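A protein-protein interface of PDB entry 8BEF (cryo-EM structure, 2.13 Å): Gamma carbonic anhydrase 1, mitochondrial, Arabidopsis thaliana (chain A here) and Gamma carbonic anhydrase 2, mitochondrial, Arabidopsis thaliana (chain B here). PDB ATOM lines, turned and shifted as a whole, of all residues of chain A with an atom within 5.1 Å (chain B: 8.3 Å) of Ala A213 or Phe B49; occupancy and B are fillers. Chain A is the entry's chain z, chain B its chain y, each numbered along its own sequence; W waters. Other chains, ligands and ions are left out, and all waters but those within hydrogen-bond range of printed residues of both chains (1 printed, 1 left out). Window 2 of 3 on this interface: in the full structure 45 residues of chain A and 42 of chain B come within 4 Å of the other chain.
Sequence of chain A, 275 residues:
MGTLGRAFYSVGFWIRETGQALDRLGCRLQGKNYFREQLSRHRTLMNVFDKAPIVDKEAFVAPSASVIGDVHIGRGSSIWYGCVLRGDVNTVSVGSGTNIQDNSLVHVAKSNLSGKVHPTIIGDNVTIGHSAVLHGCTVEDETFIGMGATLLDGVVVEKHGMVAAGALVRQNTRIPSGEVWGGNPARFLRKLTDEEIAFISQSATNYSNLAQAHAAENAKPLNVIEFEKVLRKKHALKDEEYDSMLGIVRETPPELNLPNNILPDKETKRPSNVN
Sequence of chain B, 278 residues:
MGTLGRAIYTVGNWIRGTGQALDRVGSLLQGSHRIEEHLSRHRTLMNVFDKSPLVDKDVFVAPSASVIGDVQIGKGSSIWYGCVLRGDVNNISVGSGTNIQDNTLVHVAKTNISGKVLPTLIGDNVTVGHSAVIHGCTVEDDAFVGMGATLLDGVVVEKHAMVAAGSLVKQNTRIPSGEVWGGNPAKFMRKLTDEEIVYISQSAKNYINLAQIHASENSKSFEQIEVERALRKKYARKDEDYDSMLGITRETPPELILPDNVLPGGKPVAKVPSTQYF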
ATOM      1  N   ASN A 209       2.196  -8.874 -22.164  1.00  0.00           N
ATOM      2  CA  ASN A 209       1.505 -10.048 -21.568  1.00  0.00           C
ATOM      3  C   ASN A 209      -0.009  -9.969 -21.798  1.00  0.00           C
ATOM      4  O   ASN A 209      -0.592 -11.001 -22.148  1.00  0.00           O
ATOM      5  CB  ASN A 209       1.740 -10.211 -20.063  1.00  0.00           C
ATOM      6  CG  ASN A 209       3.212 -10.267 -19.741  1.00  0.00           C
ATOM      7  OD1 ASN A 209       4.016 -10.599 -20.602  1.00  0.00           O
ATOM      8  ND2 ASN A 209       3.569  -9.847 -18.545  1.00  0.00           N
ATOM      9  N   LEU A 210      -0.580  -8.807 -21.569  1.00  0.00           N
ATOM     10  CA  LEU A 210      -2.020  -8.583 -21.838  1.00  0.00           C
ATOM     11  C   LEU A 210      -2.275  -8.833 -23.336  1.00  0.00           C
ATOM     12  O   LEU A 210      -3.216  -9.527 -23.605  1.00  0.00           O
ATOM     13  CB  LEU A 210      -2.370  -7.169 -21.362  1.00  0.00           C
ATOM     14  CG  LEU A 210      -3.839  -6.761 -21.284  1.00  0.00           C
ATOM     15  CD1 LEU A 210      -4.626  -7.696 -20.379  1.00  0.00           C
ATOM     16  CD2 LEU A 210      -3.935  -5.332 -20.770  1.00  0.00           C
ATOM     17  N   ALA A 211      -1.438  -8.285 -24.226  1.00  0.00           N
ATOM     18  CA  ALA A 211      -1.514  -8.560 -25.690  1.00  0.00           C
ATOM     19  C   ALA A 211      -1.613 -10.076 -25.890  1.00  0.00           C
ATOM     20  O   ALA A 211      -2.594 -10.462 -26.460  1.00  0.00           O
ATOM     21  CB  ALA A 211      -0.413  -7.907 -26.509  1.00  0.00           C
ATOM     22  N   GLN A 212      -0.662 -10.843 -25.321  1.00  0.00           N
ATOM     23  CA  GLN A 212      -0.689 -12.302 -25.449  1.00  0.00           C
ATOM     24  C   GLN A 212      -2.060 -12.869 -25.097  1.00  0.00           C
ATOM     25  O   GLN A 212      -2.621 -13.693 -25.838  1.00  0.00           O
ATOM     26  CB  GLN A 212       0.387 -12.931 -24.561  1.00  0.00           C
ATOM     27  CG  GLN A 212       1.682 -13.263 -25.262  1.00  0.00           C
ATOM     28  CD  GLN A 212       2.049 -12.264 -26.329  1.00  0.00           C
ATOM     29  OE1 GLN A 212       2.635 -11.223 -26.047  1.00  0.00           O
ATOM     30  NE2 GLN A 212       1.727 -12.589 -27.574  1.00  0.00           N
ATOM     31  N   ALA A 213      -2.615 -12.432 -23.965  1.00  0.00           N
ATOM     32  CA  ALA A 213      -3.918 -12.951 -23.550  1.00  0.00           C
ATOM     33  C   ALA A 213      -5.002 -12.623 -24.575  1.00  0.00           C
ATOM     34  O   ALA A 213      -5.816 -13.487 -24.932  1.00  0.00           O
ATOM     35  CB  ALA A 213      -4.295 -12.402 -22.175  1.00  0.00           C
ATOM     36  N   HIS A 214      -5.016 -11.387 -25.077  1.00  0.00           N
ATOM     37  CA  HIS A 214      -6.053 -11.000 -26.033  1.00  0.00           C
ATOM     38  C   HIS A 214      -5.866 -11.678 -27.385  1.00  0.00           C
ATOM     39  O   HIS A 214      -6.853 -11.978 -28.064  1.00  0.00           O
ATOM     40  CB  HIS A 214      -6.087  -9.482 -26.196  1.00  0.00           C
ATOM     41  CG  HIS A 214      -6.829  -8.779 -25.104  1.00  0.00           C
ATOM     42  ND1 HIS A 214      -8.070  -8.213 -25.292  1.00  0.00           N
ATOM     43  CD2 HIS A 214      -6.506  -8.556 -23.808  1.00  0.00           C
ATOM     44  CE1 HIS A 214      -8.480  -7.670 -24.159  1.00  0.00           C
ATOM     45  NE2 HIS A 214      -7.549  -7.864 -23.243  1.00  0.00           N
ATOM     46  N   ALA A 215      -4.620 -11.911 -27.802  1.00  0.00           N
ATOM     47  CA  ALA A 215      -4.376 -12.629 -29.047  1.00  0.00           C
ATOM     48  C   ALA A 215      -4.873 -14.061 -28.952  1.00  0.00           C
ATOM     49  O   ALA A 215      -5.459 -14.585 -29.904  1.00  0.00           O
ATOM     50  CB  ALA A 215      -2.889 -12.596 -29.400  1.00  0.00           C
ATOM     51  N   ALA A 216      -4.648 -14.709 -27.806  1.00  0.00           N
ATOM     52  CA  ALA A 216      -5.196 -16.049 -27.618  1.00  0.00           C
ATOM     53  C   ALA A 216      -6.721 -16.026 -27.616  1.00  0.00           C
ATOM     54  O   ALA A 216      -7.363 -16.910 -28.195  1.00  0.00           O
ATOM     55  CB  ALA A 216      -4.657 -16.661 -26.326  1.00  0.00           C
ATOM     56  N   GLU A 217      -7.322 -15.021 -26.971  1.00  0.00           N
ATOM     57  CA  GLU A 217      -8.779 -14.907 -26.970  1.00  0.00           C
ATOM     58  C   GLU A 217      -9.327 -14.778 -28.390  1.00  0.00           C
ATOM     59  O   GLU A 217     -10.249 -15.502 -28.780  1.00  0.00           O
ATOM     60  CB  GLU A 217      -9.210 -13.703 -26.128  1.00  0.00           C
ATOM     61  CG  GLU A 217      -9.499 -13.992 -24.655  1.00  0.00           C
ATOM     62  CD  GLU A 217     -10.428 -15.169 -24.428  1.00  0.00           C
ATOM     63  OE1 GLU A 217     -11.311 -15.424 -25.272  1.00  0.00           O
ATOM     64  OE2 GLU A 217     -10.283 -15.839 -23.386  1.00  0.00           O
ATOM     65  N   MET B  46     -16.812 -10.248 -25.992  1.00  0.00           N
ATOM     66  CA  MET B  46     -15.733 -11.218 -25.885  1.00  0.00           C
ATOM     67  C   MET B  46     -15.361 -11.453 -24.430  1.00  0.00           C
ATOM     68  O   MET B  46     -15.355 -10.523 -23.621  1.00  0.00           O
ATOM     69  CB  MET B  46     -14.488 -10.766 -26.653  1.00  0.00           C
ATOM     70  CG  MET B  46     -13.605 -11.915 -27.109  1.00  0.00           C
ATOM     71  SD  MET B  46     -12.225 -11.368 -28.125  1.00  0.00           S
ATOM     72  CE  MET B  46     -11.296 -10.412 -26.925  1.00  0.00           C
ATOM     73  N   ASN B  47     -15.042 -12.702 -24.115  1.00  0.00           N
ATOM     74  CA  ASN B  47     -14.482 -13.044 -22.820  1.00  0.00           C
ATOM     75  C   ASN B  47     -12.987 -12.761 -22.803  1.00  0.00           C
ATOM     76  O   ASN B  47     -12.323 -12.756 -23.842  1.00  0.00           O
ATOM     77  CB  ASN B  47     -14.707 -14.520 -22.496  1.00  0.00           C
ATOM     78  CG  ASN B  47     -16.144 -14.934 -22.640  1.00  0.00           C
ATOM     79  OD1 ASN B  47     -16.944 -14.763 -21.728  1.00  0.00           O
ATOM     80  ND2 ASN B  47     -16.484 -15.487 -23.795  1.00  0.00           N
ATOM     81  N   VAL B  48     -12.464 -12.514 -21.608  1.00  0.00           N
ATOM     82  CA  VAL B  48     -11.025 -12.539 -21.373  1.00  0.00           C
ATOM     83  C   VAL B  48     -10.810 -12.826 -19.894  1.00  0.00           C
ATOM     84  O   VAL B  48     -11.551 -12.330 -19.042  1.00  0.00           O
ATOM     85  CB  VAL B  48     -10.338 -11.227 -21.819  1.00  0.00           C
ATOM     86  CG1 VAL B  48     -10.906 -10.029 -21.081  1.00  0.00           C
ATOM     87  CG2 VAL B  48      -8.827 -11.322 -21.650  1.00  0.00           C
ATOM     88  N   PHE B  49      -9.809 -13.656 -19.597  1.00  0.00           N
ATOM     89  CA  PHE B  49      -9.505 -14.065 -18.223  1.00  0.00           C
ATOM     90  C   PHE B  49     -10.728 -14.675 -17.544  1.00  0.00           C
ATOM     91  O   PHE B  49     -10.959 -14.488 -16.348  1.00  0.00           O
ATOM     92  CB  PHE B  49      -8.964 -12.893 -17.404  1.00  0.00           C
ATOM     93  CG  PHE B  49      -7.722 -12.281 -17.967  1.00  0.00           C
ATOM     94  CD1 PHE B  49      -6.631 -13.070 -18.287  1.00  0.00           C
ATOM     95  CD2 PHE B  49      -7.638 -10.915 -18.164  1.00  0.00           C
ATOM     96  CE1 PHE B  49      -5.481 -12.511 -18.801  1.00  0.00           C
ATOM     97  CE2 PHE B  49      -6.493 -10.348 -18.676  1.00  0.00           C
ATOM     98  CZ  PHE B  49      -5.411 -11.148 -18.998  1.00  0.00           C
ATOM     99  N   ASP B  50     -11.517 -15.417 -18.322  1.00  0.00           N
ATOM    100  CA  ASP B  50     -12.747 -16.049 -17.837  1.00  0.00           C
ATOM    101  C   ASP B  50     -13.698 -15.031 -17.212  1.00  0.00           C
ATOM    102  O   ASP B  50     -14.331 -15.292 -16.188  1.00  0.00           O
ATOM    103  CB  ASP B  50     -12.443 -17.183 -16.854  1.00  0.00           C
ATOM    104  CG  ASP B  50     -11.836 -18.396 -17.528  1.00  0.00           C
ATOM    105  OD1 ASP B  50     -11.906 -18.489 -18.772  1.00  0.00           O
ATOM    106  OD2 ASP B  50     -11.287 -19.261 -16.813  1.00  0.00           O
ATOM    107  N   LYS B  51     -13.791 -13.854 -17.823  1.00  0.00           N
ATOM    108  CA  LYS B  51     -14.772 -12.846 -17.447  1.00  0.00           C
ATOM    109  C   LYS B  51     -15.679 -12.584 -18.639  1.00  0.00           C
ATOM    110  O   LYS B  51     -15.198 -12.269 -19.731  1.00  0.00           O
ATOM    111  CB  LYS B  51     -14.099 -11.548 -16.990  1.00  0.00           C
ATOM    112  CG  LYS B  51     -13.296 -11.676 -15.711  1.00  0.00           C
ATOM    113  CD  LYS B  51     -14.201 -11.658 -14.489  1.00  0.00           C
ATOM    114  CE  LYS B  51     -13.489 -12.205 -13.262  1.00  0.00           C
ATOM    115  NZ  LYS B  51     -13.487 -11.229 -12.138  1.00  0.00           N
ATOM    116  N   SER B  52     -16.982 -12.715 -18.428  1.00  0.00           N
ATOM    117  CA  SER B  52     -17.963 -12.510 -19.479  1.00  0.00           C
ATOM    118  C   SER B  52     -18.730 -11.225 -19.235  1.00  0.00           C
ATOM    119  O   SER B  52     -19.147 -10.971 -18.097  1.00  0.00           O
ATOM    120  CB  SER B  52     -18.936 -13.689 -19.541  1.00  0.00           C
ATOM    121  OG  SER B  52     -19.435 -13.869 -20.851  1.00  0.00           O
ATOM    122  N   ILE B  68     -15.559  -6.077 -23.836  1.00  0.00           N
ATOM    123  CA  ILE B  68     -14.571  -7.114 -23.571  1.00  0.00           C
ATOM    124  C   ILE B  68     -14.423  -7.299 -22.067  1.00  0.00           C
ATOM    125  O   ILE B  68     -14.207  -6.328 -21.336  1.00  0.00           O
ATOM    126  CB  ILE B  68     -13.211  -6.768 -24.203  1.00  0.00           C
ATOM    127  CG1 ILE B  68     -13.290  -6.878 -25.727  1.00  0.00           C
ATOM    128  CG2 ILE B  68     -12.133  -7.690 -23.671  1.00  0.00           C
ATOM    129  CD1 ILE B  68     -12.287  -6.024 -26.449  1.00  0.00           C
ATOM    130  N   GLY B  69     -14.519  -8.545 -21.614  1.00  0.00           N
ATOM    131  CA  GLY B  69     -14.186  -8.887 -20.247  1.00  0.00           C
ATOM    132  C   GLY B  69     -15.266  -8.618 -19.220  1.00  0.00           C
ATOM    133  O   GLY B  69     -16.442  -8.917 -19.442  1.00  0.00           O
ATOM    134  N   ASP B  70     -14.865  -8.046 -18.086  1.00  0.00           N
ATOM    135  CA  ASP B  70     -15.746  -7.887 -16.930  1.00  0.00           C
ATOM    136  C   ASP B  70     -16.451  -6.535 -17.033  1.00  0.00           C
ATOM    137  O   ASP B  70     -16.063  -5.539 -16.421  1.00  0.00           O
ATOM    138  CB  ASP B  70     -14.946  -8.032 -15.639  1.00  0.00           C
ATOM    139  CG  ASP B  70     -15.766  -7.735 -14.404  1.00  0.00           C
ATOM    140  OD1 ASP B  70     -16.999  -7.916 -14.447  1.00  0.00           O
ATOM    141  OD2 ASP B  70     -15.174  -7.331 -13.384  1.00  0.00           O
ATOM    142  N   ARG B  86     -13.184  -1.986 -22.487  1.00  0.00           N
ATOM    143  CA  ARG B  86     -12.221  -3.056 -22.242  1.00  0.00           C
ATOM    144  C   ARG B  86     -12.098  -3.340 -20.737  1.00  0.00           C
ATOM    145  O   ARG B  86     -11.369  -2.714 -20.078  1.00  0.00           O
ATOM    146  CB  ARG B  86     -10.905  -2.720 -22.959  1.00  0.00           C
ATOM    147  CG  ARG B  86      -9.838  -3.796 -22.828  1.00  0.00           C
ATOM    148  CD  ARG B  86      -8.843  -3.829 -23.964  1.00  0.00           C
ATOM    149  NE  ARG B  86      -8.021  -2.651 -24.173  1.00  0.00           N
ATOM    150  CZ  ARG B  86      -6.822  -2.442 -23.647  1.00  0.00           C
ATOM    151  NH1 ARG B  86      -6.282  -3.327 -22.836  1.00  0.00           N
ATOM    152  NH2 ARG B  86      -6.162  -1.341 -23.936  1.00  0.00           N
ATOM    153  N   GLY B  87     -12.896  -4.217 -20.243  1.00  0.00           N
ATOM    154  CA  GLY B  87     -12.825  -4.592 -18.843  1.00  0.00           C
ATOM    155  C   GLY B  87     -11.960  -5.814 -18.611  1.00  0.00           C
ATOM    156  O   GLY B  87     -12.461  -6.844 -18.154  1.00  0.00           O
ATOM    157  N   ASP B  88     -10.666  -5.726 -18.917  1.00  0.00           N
ATOM    158  CA  ASP B  88      -9.812  -6.908 -18.864  1.00  0.00           C
ATOM    159  C   ASP B  88      -9.033  -7.044 -17.561  1.00  0.00           C
ATOM    160  O   ASP B  88      -8.952  -8.147 -17.018  1.00  0.00           O
ATOM    161  CB  ASP B  88      -8.835  -6.928 -20.048  1.00  0.00           C
ATOM    162  CG  ASP B  88      -8.148  -5.597 -20.278  1.00  0.00           C
ATOM    163  OD1 ASP B  88      -8.248  -4.698 -19.419  1.00  0.00           O
ATOM    164  OD2 ASP B  88      -7.498  -5.457 -21.331  1.00  0.00           O
ATOM    165  N   VAL B  89      -8.457  -5.994 -16.993  1.00  0.00           N
ATOM    166  CA  VAL B  89      -7.655  -6.088 -15.719  1.00  0.00           C
ATOM    167  C   VAL B  89      -8.509  -5.653 -14.507  1.00  0.00           C
ATOM    168  O   VAL B  89      -8.116  -5.912 -13.419  1.00  0.00           O
ATOM    169  CB  VAL B  89      -6.322  -5.317 -15.819  1.00  0.00           C
ATOM    170  CG1 VAL B  89      -5.519  -5.821 -17.012  1.00  0.00           C
ATOM    171  CG2 VAL B  89      -6.541  -3.817 -15.957  1.00  0.00           C
ATOM    172  N   ASN B  90      -9.691  -5.114 -14.755  1.00  0.00           N
ATOM    173  CA  ASN B  90     -10.569  -4.570 -13.701  1.00  0.00           C
ATOM    174  C   ASN B  90     -12.008  -4.498 -14.203  1.00  0.00           C
ATOM    175  O   ASN B  90     -12.214  -4.808 -15.333  1.00  0.00           O
ATOM    176  CB  ASN B  90      -9.989  -3.235 -13.208  1.00  0.00           C
ATOM    177  CG  ASN B  90     -10.220  -3.007 -11.731  1.00  0.00           C
ATOM    178  OD1 ASN B  90     -11.100  -3.610 -11.144  1.00  0.00           O
ATOM    179  ND2 ASN B  90      -9.457  -2.122 -11.121  1.00  0.00           N
HETATM  180  O   HOH W   1     -12.674 -15.049 -28.490  1.00  0.00           O
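The backbone NH (N) of Gly B69 lies within hydrogen-bond range of the backbone carbonyl oxygen (O) of Met B46. The side-chain hydroxyl (OG) of Ser B52 sits at hydrogen-bond distance from the side-chain amide oxygen (OD1) of Asn B47, 2.8 Å away. The backbone carbonyl oxygen of Ile B68 sits at hydrogen-bond distance from the backbone NH of Gly B87, 2.7 Å away. The guanidinium group of Arg B86 lies within salt-bridge range of the side-chain carboxylate of Asp B88 (2.9 Å).
Ala A213 touches just one residue of chain B: Phe B49 (3.6 Å). Phe B49 touches just these residues of chain A: Leu A210 (3.7 Å) and Ala A213 (3.6 Å). Of the printed residues of chain A, Met B46 touches Glu A217. Of the printed residues of chain B, His A214 touches Ile B68 (3.7 Å), Arg B86 (3.9 Å) and Asp B88 (3.1 Å). Of the printed residues of chain A, Val B89 touches Leu A210 (3.96 Å). Printed residues of chain A within 4 Å of Ile B68: His A214. Of the printed residues of chain A, Asn B47 touches Glu A217 (3.1 Å). Ser B52 touches none of the printed residues of chain A. Gly B87 touches none of the printed residues of chain A. The nearest printed residue of chain A that does not touch Met B46 is His A214 (4.2 Å).
Leu A210 touches Phe B49 (CD1 to CE2, 3.7 Å). Arg B86 touches Leu A210 (NH1 to CD2, 3.7 Å). CD2 of Leu A210 touches OD2 of Asp B88, 3.6 Å away. Val B89 touches Leu A210 (CG1 to CD1, 3.96 Å). CE1 of Phe B49 touches CB of Ala A213, 3.6 Å away. Ile B68 touches His A214. His A214 touches Arg B86. CB of Glu A217 touches CE of Met B46, 3.98 Å away. Glu A217 touches Val B48.
Hydrophobic or aromatic side chains of chain B that line the printed part of chain A: Met B46, Phe B49, Ile B68 and Val B89. Along chain B the printed residues that touch a printed residue of chain A span positions 46 to 89. Of the 9 printed residues of chain A, 4 touch a printed residue of chain B. Among the printed residues, 11 pairs touch across the chains.
Water W1 bridges the backbone carbonyl oxygen of Glu A217 (2.5 Å) and the side-chain sulfur of Met B46 (3.7 Å).
OD2 of Asp B88 sits at hydrogen-bond distance from NE2 of His A214, 3.1 Å away. OE1 of Glu A217 lies close to O of Asn B47 (3.2 Å).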
